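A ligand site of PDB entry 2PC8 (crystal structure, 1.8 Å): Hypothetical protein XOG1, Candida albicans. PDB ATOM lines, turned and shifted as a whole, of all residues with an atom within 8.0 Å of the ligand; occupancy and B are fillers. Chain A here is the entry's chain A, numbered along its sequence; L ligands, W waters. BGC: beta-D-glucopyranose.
The backbone NH (N) of Ser 285 lies close to the side-chain amide nitrogen (ND2) of Asn 236 (3.1 Å). The side-chain carboxylate (OD1) of Asp 11 sits at hydrogen-bond distance from the indole nitrogen (NE1) of Trp 287 (3.0 Å). N of Val 250 lies within hydrogen-bond range of O of Trp 287 (2.9 Å). The backbone carbonyl oxygen (O) of Asn 247 lies within hydrogen-bond range of the backbone NH (N) of Val 223. The guanidinium group of Arg 215 is in hydrogen-bond range of the backbone carbonyl oxygen of Asn 247, at 3.3 Å. O of Phe 238 lies within hydrogen-bond range of NE2 of His 286, at 2.8 Å. The backbone NH of Trp 246 is in hydrogen-bond range of the side-chain hydroxyl of Tyr 211, at 3.0 Å. O of Trp 246 is in hydrogen-bond range of NH2 of Arg 215, 2.9 Å away.
CG2 of Val 241 touches C2 of the ligand (3.9 Å). Trp 246 touches the ligand. His 286 touches the ligand. Hydrophobic or aromatic side chains within 4 Å of the ligand: Val 241, Trp 246, Val 248, His 286 and Trp 287.
Water W1 lies within hydrogen-bond range of the backbone carbonyl oxygen (O) of Gln 245 (2.8 Å), an oxygen (O3) of the ligand (2.8 Å) and the backbone carbonyl oxygen (O) of Leu 239 (2.9 Å).
The backbone carbonyl oxygen (O) of Ser 285 lies within hydrogen-bond range of an oxygen (O6) of the ligand (2.6 Å). N of Val 248 lies within hydrogen-bond range of O3 of the ligand (2.8 Å). O of Val 248 is in hydrogen-bond range of O4 of the ligand. An oxygen (O4) of the ligand lies within hydrogen-bond range of the backbone NH (N) of Trp 287 (3.0 Å). An oxygen (O2) of the ligand lies within hydrogen-bond range of the backbone NH (N) of Asn 247 (3.0 Å).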
ATOM      1  N   TYR A  10       9.355 -19.106  15.745  1.00  0.00           N
ATOM      2  CA  TYR A  10       9.319 -19.346  17.189  1.00  0.00           C
ATOM      3  C   TYR A  10       9.956 -18.191  17.963  1.00  0.00           C
ATOM      4  O   TYR A  10       9.717 -18.072  19.163  1.00  0.00           O
ATOM      5  CB  TYR A  10      10.008 -20.656  17.567  1.00  0.00           C
ATOM      6  CG  TYR A  10       9.121 -21.886  17.407  1.00  0.00           C
ATOM      7  CD1 TYR A  10       8.238 -22.272  18.417  1.00  0.00           C
ATOM      8  CD2 TYR A  10       9.191 -22.680  16.263  1.00  0.00           C
ATOM      9  CE1 TYR A  10       7.442 -23.410  18.271  1.00  0.00           C
ATOM     10  CE2 TYR A  10       8.401 -23.810  16.119  1.00  0.00           C
ATOM     11  CZ  TYR A  10       7.537 -24.171  17.123  1.00  0.00           C
ATOM     12  OH  TYR A  10       6.753 -25.294  16.980  1.00  0.00           O
ATOM     13  N   ASP A  11      10.760 -17.373  17.295  1.00  0.00           N
ATOM     14  CA  ASP A  11      11.305 -16.170  17.935  1.00  0.00           C
ATOM     15  C   ASP A  11      10.286 -15.062  18.065  1.00  0.00           C
ATOM     16  O   ASP A  11      10.292 -14.348  19.058  1.00  0.00           O
ATOM     17  CB  ASP A  11      12.508 -15.633  17.160  1.00  0.00           C
ATOM     18  CG  ASP A  11      13.719 -16.501  17.299  1.00  0.00           C
ATOM     19  OD1 ASP A  11      14.053 -16.859  18.442  1.00  0.00           O
ATOM     20  OD2 ASP A  11      14.334 -16.837  16.270  1.00  0.00           O
ATOM     21  N   TYR A 211      15.758 -37.406  17.520  1.00  0.00           N
ATOM     22  CA  TYR A 211      16.242 -36.184  16.857  1.00  0.00           C
ATOM     23  C   TYR A 211      17.043 -36.544  15.587  1.00  0.00           C
ATOM     24  O   TYR A 211      16.739 -36.090  14.507  1.00  0.00           O
ATOM     25  CB  TYR A 211      17.079 -35.324  17.819  1.00  0.00           C
ATOM     26  CG  TYR A 211      17.699 -34.142  17.103  1.00  0.00           C
ATOM     27  CD1 TYR A 211      16.999 -32.935  16.928  1.00  0.00           C
ATOM     28  CD2 TYR A 211      18.935 -34.272  16.512  1.00  0.00           C
ATOM     29  CE1 TYR A 211      17.569 -31.884  16.214  1.00  0.00           C
ATOM     30  CE2 TYR A 211      19.485 -33.254  15.782  1.00  0.00           C
ATOM     31  CZ  TYR A 211      18.811 -32.062  15.642  1.00  0.00           C
ATOM     32  OH  TYR A 211      19.385 -31.076  14.902  1.00  0.00           O
ATOM     33  N   ARG A 215      16.143 -35.900  11.434  1.00  0.00           N
ATOM     34  CA  ARG A 215      17.004 -35.049  10.603  1.00  0.00           C
ATOM     35  C   ARG A 215      17.608 -35.843   9.441  1.00  0.00           C
ATOM     36  O   ARG A 215      17.765 -35.327   8.334  1.00  0.00           O
ATOM     37  CB  ARG A 215      18.091 -34.397  11.460  1.00  0.00           C
ATOM     38  CG  ARG A 215      17.565 -33.364  12.457  1.00  0.00           C
ATOM     39  CD  ARG A 215      17.413 -31.932  11.873  1.00  0.00           C
ATOM     40  NE  ARG A 215      16.728 -31.091  12.848  1.00  0.00           N
ATOM     41  CZ  ARG A 215      15.404 -30.952  12.973  1.00  0.00           C
ATOM     42  NH1 ARG A 215      14.578 -31.520  12.102  1.00  0.00           N
ATOM     43  NH2 ARG A 215      14.909 -30.223  13.964  1.00  0.00           N
ATOM     44  N   PRO A 222      10.640 -28.935  13.487  1.00  0.00           N
ATOM     45  CA  PRO A 222      11.032 -28.869  14.884  1.00  0.00           C
ATOM     46  C   PRO A 222      10.741 -30.145  15.682  1.00  0.00           C
ATOM     47  O   PRO A 222       9.706 -30.794  15.493  1.00  0.00           O
ATOM     48  CB  PRO A 222      10.232 -27.683  15.417  1.00  0.00           C
ATOM     49  CG  PRO A 222      10.027 -26.817  14.222  1.00  0.00           C
ATOM     50  CD  PRO A 222       9.771 -27.793  13.136  1.00  0.00           C
ATOM     51  N   VAL A 223      11.711 -30.514  16.514  1.00  0.00           N
ATOM     52  CA  VAL A 223      11.583 -31.622  17.452  1.00  0.00           C
ATOM     53  C   VAL A 223      11.144 -31.055  18.812  1.00  0.00           C
ATOM     54  O   VAL A 223      11.768 -30.140  19.342  1.00  0.00           O
ATOM     55  CB  VAL A 223      12.926 -32.390  17.593  1.00  0.00           C
ATOM     56  CG1 VAL A 223      12.887 -33.378  18.780  1.00  0.00           C
ATOM     57  CG2 VAL A 223      13.265 -33.144  16.269  1.00  0.00           C
ATOM     58  N   ASN A 236      18.772 -27.313  29.426  1.00  0.00           N
ATOM     59  CA  ASN A 236      19.512 -26.218  28.770  1.00  0.00           C
ATOM     60  C   ASN A 236      20.738 -26.719  27.995  1.00  0.00           C
ATOM     61  O   ASN A 236      21.060 -26.166  26.944  1.00  0.00           O
ATOM     62  CB  ASN A 236      19.997 -25.204  29.813  1.00  0.00           C
ATOM     63  CG  ASN A 236      18.928 -24.226  30.267  1.00  0.00           C
ATOM     64  OD1 ASN A 236      19.184 -23.435  31.184  1.00  0.00           O
ATOM     65  ND2 ASN A 236      17.749 -24.247  29.658  1.00  0.00           N
ATOM     66  N   PHE A 238      21.238 -29.743  26.612  1.00  0.00           N
ATOM     67  CA  PHE A 238      20.913 -30.903  25.797  1.00  0.00           C
ATOM     68  C   PHE A 238      20.333 -30.436  24.456  1.00  0.00           C
ATOM     69  O   PHE A 238      19.525 -29.533  24.433  1.00  0.00           O
ATOM     70  CB  PHE A 238      19.885 -31.761  26.569  1.00  0.00           C
ATOM     71  CG  PHE A 238      19.525 -33.047  25.892  1.00  0.00           C
ATOM     72  CD1 PHE A 238      20.428 -34.095  25.829  1.00  0.00           C
ATOM     73  CD2 PHE A 238      18.268 -33.225  25.354  1.00  0.00           C
ATOM     74  CE1 PHE A 238      20.078 -35.308  25.210  1.00  0.00           C
ATOM     75  CE2 PHE A 238      17.924 -34.430  24.736  1.00  0.00           C
ATOM     76  CZ  PHE A 238      18.846 -35.455  24.677  1.00  0.00           C
ATOM     77  N   LEU A 239      20.746 -31.065  23.363  1.00  0.00           N
ATOM     78  CA  LEU A 239      20.275 -30.688  22.010  1.00  0.00           C
ATOM     79  C   LEU A 239      20.522 -29.198  21.735  1.00  0.00           C
ATOM     80  O   LEU A 239      19.595 -28.398  21.584  1.00  0.00           O
ATOM     81  CB  LEU A 239      18.804 -31.091  21.767  1.00  0.00           C
ATOM     82  CG  LEU A 239      18.567 -32.589  21.646  1.00  0.00           C
ATOM     83  CD1 LEU A 239      17.062 -32.877  21.600  1.00  0.00           C
ATOM     84  CD2 LEU A 239      19.288 -33.169  20.433  1.00  0.00           C
ATOM     85  N   THR A 240      21.813 -28.842  21.673  1.00  0.00           N
ATOM     86  CA  THR A 240      22.209 -27.454  21.648  1.00  0.00           C
ATOM     87  C   THR A 240      22.837 -27.089  20.315  1.00  0.00           C
ATOM     88  O   THR A 240      23.377 -27.934  19.622  1.00  0.00           O
ATOM     89  CB  THR A 240      23.219 -27.138  22.760  1.00  0.00           C
ATOM     90  OG1 THR A 240      24.421 -27.884  22.537  1.00  0.00           O
ATOM     91  CG2 THR A 240      22.635 -27.483  24.146  1.00  0.00           C
ATOM     92  N   VAL A 241      22.724 -25.801  19.992  1.00  0.00           N
ATOM     93  CA  VAL A 241      23.347 -25.228  18.794  1.00  0.00           C
ATOM     94  C   VAL A 241      24.869 -25.455  18.825  1.00  0.00           C
ATOM     95  O   VAL A 241      25.471 -25.728  17.802  1.00  0.00           O
ATOM     96  CB  VAL A 241      22.992 -23.731  18.690  1.00  0.00           C
ATOM     97  CG1 VAL A 241      23.930 -22.962  17.718  1.00  0.00           C
ATOM     98  CG2 VAL A 241      21.517 -23.585  18.273  1.00  0.00           C
ATOM     99  N   GLN A 245      22.766 -29.083  16.882  1.00  0.00           N
ATOM    100  CA  GLN A 245      21.419 -29.604  17.032  1.00  0.00           C
ATOM    101  C   GLN A 245      20.502 -28.402  17.114  1.00  0.00           C
ATOM    102  O   GLN A 245      20.721 -27.522  17.932  1.00  0.00           O
ATOM    103  CB  GLN A 245      21.354 -30.523  18.259  1.00  0.00           C
ATOM    104  CG  GLN A 245      22.207 -31.775  18.088  1.00  0.00           C
ATOM    105  CD  GLN A 245      22.820 -32.328  19.374  1.00  0.00           C
ATOM    106  OE1 GLN A 245      22.849 -31.666  20.404  1.00  0.00           O
ATOM    107  NE2 GLN A 245      23.333 -33.545  19.295  1.00  0.00           N
ATOM    108  N   TRP A 246      19.477 -28.351  16.249  1.00  0.00           N
ATOM    109  CA  TRP A 246      18.747 -27.127  15.968  1.00  0.00           C
ATOM    110  C   TRP A 246      17.268 -27.456  15.723  1.00  0.00           C
ATOM    111  O   TRP A 246      16.910 -28.606  15.399  1.00  0.00           O
ATOM    112  CB  TRP A 246      19.362 -26.350  14.769  1.00  0.00           C
ATOM    113  CG  TRP A 246      19.403 -27.184  13.545  1.00  0.00           C
ATOM    114  CD1 TRP A 246      20.298 -28.162  13.262  1.00  0.00           C
ATOM    115  CD2 TRP A 246      18.444 -27.197  12.493  1.00  0.00           C
ATOM    116  NE1 TRP A 246      19.962 -28.774  12.077  1.00  0.00           N
ATOM    117  CE2 TRP A 246      18.835 -28.183  11.582  1.00  0.00           C
ATOM    118  CE3 TRP A 246      17.298 -26.428  12.220  1.00  0.00           C
ATOM    119  CZ2 TRP A 246      18.108 -28.453  10.414  1.00  0.00           C
ATOM    120  CZ3 TRP A 246      16.592 -26.690  11.052  1.00  0.00           C
ATOM    121  CH2 TRP A 246      16.996 -27.705  10.174  1.00  0.00           C
ATOM    122  N   ASN A 247      16.424 -26.434  15.877  1.00  0.00           N
ATOM    123  CA  ASN A 247      14.981 -26.528  15.781  1.00  0.00           C
ATOM    124  C   ASN A 247      14.439 -27.488  16.835  1.00  0.00           C
ATOM    125  O   ASN A 247      13.789 -28.486  16.534  1.00  0.00           O
ATOM    126  CB  ASN A 247      14.485 -26.913  14.366  1.00  0.00           C
ATOM    127  CG  ASN A 247      14.084 -25.717  13.530  1.00  0.00           C
ATOM    128  OD1 ASN A 247      14.332 -24.563  13.916  1.00  0.00           O
ATOM    129  ND2 ASN A 247      13.456 -25.968  12.378  1.00  0.00           N
ATOM    130  N   VAL A 248      14.752 -27.158  18.087  1.00  0.00           N
ATOM    131  CA  VAL A 248      14.364 -27.964  19.247  1.00  0.00           C
ATOM    132  C   VAL A 248      13.522 -27.087  20.173  1.00  0.00           C
ATOM    133  O   VAL A 248      13.897 -25.963  20.488  1.00  0.00           O
ATOM    134  CB  VAL A 248      15.616 -28.512  19.958  1.00  0.00           C
ATOM    135  CG1 VAL A 248      15.260 -29.186  21.272  1.00  0.00           C
ATOM    136  CG2 VAL A 248      16.348 -29.506  19.024  1.00  0.00           C
ATOM    137  N   VAL A 249      12.398 -27.614  20.653  1.00  0.00           N
ATOM    138  CA  VAL A 249      11.496 -26.876  21.529  1.00  0.00           C
ATOM    139  C   VAL A 249      11.248 -27.745  22.754  1.00  0.00           C
ATOM    140  O   VAL A 249      11.079 -28.955  22.615  1.00  0.00           O
ATOM    141  CB  VAL A 249      10.140 -26.555  20.813  1.00  0.00           C
ATOM    142  CG1 VAL A 249       9.146 -25.856  21.750  1.00  0.00           C
ATOM    143  CG2 VAL A 249      10.360 -25.721  19.540  1.00  0.00           C
ATOM    144  N   VAL A 250      11.214 -27.147  23.929  1.00  0.00           N
ATOM    145  CA  VAL A 250      10.871 -27.857  25.160  1.00  0.00           C
ATOM    146  C   VAL A 250       9.423 -27.535  25.529  1.00  0.00           C
ATOM    147  O   VAL A 250       8.981 -26.376  25.515  1.00  0.00           O
ATOM    148  CB  VAL A 250      11.797 -27.451  26.323  1.00  0.00           C
ATOM    149  CG1 VAL A 250      11.321 -28.119  27.660  1.00  0.00           C
ATOM    150  CG2 VAL A 250      13.265 -27.820  25.972  1.00  0.00           C
ATOM    151  N   GLU A 284      15.429 -20.039  30.374  1.00  0.00           N
ATOM    152  CA  GLU A 284      15.905 -21.228  29.684  1.00  0.00           C
ATOM    153  C   GLU A 284      16.485 -20.906  28.304  1.00  0.00           C
ATOM    154  O   GLU A 284      16.134 -19.909  27.693  1.00  0.00           O
ATOM    155  CB  GLU A 284      14.782 -22.245  29.526  1.00  0.00           C
ATOM    156  CG  GLU A 284      14.314 -22.796  30.840  1.00  0.00           C
ATOM    157  CD  GLU A 284      13.325 -23.949  30.657  1.00  0.00           C
ATOM    158  OE1 GLU A 284      12.476 -23.831  29.761  1.00  0.00           O
ATOM    159  OE2 GLU A 284      13.436 -24.950  31.402  1.00  0.00           O
ATOM    160  N   SER A 285      17.322 -21.798  27.809  1.00  0.00           N
ATOM    161  CA  SER A 285      18.042 -21.580  26.566  1.00  0.00           C
ATOM    162  C   SER A 285      17.381 -22.183  25.320  1.00  0.00           C
ATOM    163  O   SER A 285      17.900 -21.990  24.223  1.00  0.00           O
ATOM    164  CB  SER A 285      19.461 -22.119  26.695  1.00  0.00           C
ATOM    165  OG  SER A 285      19.435 -23.521  26.899  1.00  0.00           O
ATOM    166  N   HIS A 286      16.309 -22.951  25.467  1.00  0.00           N
ATOM    167  CA  HIS A 286      15.537 -23.395  24.301  1.00  0.00           C
ATOM    168  C   HIS A 286      14.250 -22.656  24.210  1.00  0.00           C
ATOM    169  O   HIS A 286      13.702 -22.227  25.214  1.00  0.00           O
ATOM    170  CB  HIS A 286      15.151 -24.872  24.334  1.00  0.00           C
ATOM    171  CG  HIS A 286      16.300 -25.814  24.285  1.00  0.00           C
ATOM    172  ND1 HIS A 286      16.885 -26.231  23.104  1.00  0.00           N
ATOM    173  CD2 HIS A 286      16.972 -26.434  25.279  1.00  0.00           C
ATOM    174  CE1 HIS A 286      17.862 -27.084  23.392  1.00  0.00           C
ATOM    175  NE2 HIS A 286      17.934 -27.220  24.697  1.00  0.00           N
ATOM    176  N   TRP A 287      13.742 -22.534  22.984  1.00  0.00           N
ATOM    177  CA  TRP A 287      12.357 -22.178  22.755  1.00  0.00           C
ATOM    178  C   TRP A 287      11.501 -23.117  23.615  1.00  0.00           C
ATOM    179  O   TRP A 287      11.821 -24.281  23.722  1.00  0.00           O
ATOM    180  CB  TRP A 287      11.991 -22.402  21.296  1.00  0.00           C
ATOM    181  CG  TRP A 287      12.599 -21.471  20.322  1.00  0.00           C
ATOM    182  CD1 TRP A 287      12.857 -20.144  20.491  1.00  0.00           C
ATOM    183  CD2 TRP A 287      12.912 -21.785  18.964  1.00  0.00           C
ATOM    184  NE1 TRP A 287      13.372 -19.615  19.313  1.00  0.00           N
ATOM    185  CE2 TRP A 287      13.405 -20.607  18.361  1.00  0.00           C
ATOM    186  CE3 TRP A 287      12.855 -22.959  18.203  1.00  0.00           C
ATOM    187  CZ2 TRP A 287      13.839 -20.567  17.028  1.00  0.00           C
ATOM    188  CZ3 TRP A 287      13.268 -22.915  16.883  1.00  0.00           C
ATOM    189  CH2 TRP A 287      13.763 -21.731  16.313  1.00  0.00           C
ATOM    190  N   ASN A 288      10.453 -22.592  24.214  1.00  0.00           N
ATOM    191  CA  ASN A 288       9.590 -23.406  25.075  1.00  0.00           C
ATOM    192  C   ASN A 288       8.134 -22.928  25.028  1.00  0.00           C
ATOM    193  O   ASN A 288       7.868 -21.740  24.818  1.00  0.00           O
ATOM    194  CB  ASN A 288      10.111 -23.444  26.518  1.00  0.00           C
ATOM    195  CG  ASN A 288      10.176 -22.074  27.171  1.00  0.00           C
ATOM    196  OD1 ASN A 288       9.211 -21.640  27.811  1.00  0.00           O
ATOM    197  ND2 ASN A 288      11.316 -21.372  26.990  1.00  0.00           N
HETATM  198  C2  BGC L   1      17.673 -23.240  17.792  1.00  0.00           C
HETATM  199  C3  BGC L   1      16.586 -23.857  18.692  1.00  0.00           C
HETATM  200  C4  BGC L   1      16.574 -23.194  20.077  1.00  0.00           C
HETATM  201  C5  BGC L   1      16.504 -21.666  19.923  1.00  0.00           C
HETATM  202  C6  BGC L   1      16.560 -20.933  21.258  1.00  0.00           C
HETATM  203  C1  BGC L   1      17.513 -21.722  17.758  1.00  0.00           C
HETATM  204  O1  BGC L   1      18.542 -21.155  16.976  1.00  0.00           O
HETATM  205  O2  BGC L   1      17.581 -23.747  16.476  1.00  0.00           O
HETATM  206  O3  BGC L   1      16.737 -25.246  18.790  1.00  0.00           O
HETATM  207  O4  BGC L   1      15.504 -23.692  20.891  1.00  0.00           O
HETATM  208  O5  BGC L   1      17.552 -21.184  19.077  1.00  0.00           O
HETATM  209  O6  BGC L   1      17.842 -21.046  21.825  1.00  0.00           O
HETATM  210  O   HOH W   1      19.115 -26.242  19.772  1.00  0.00           O
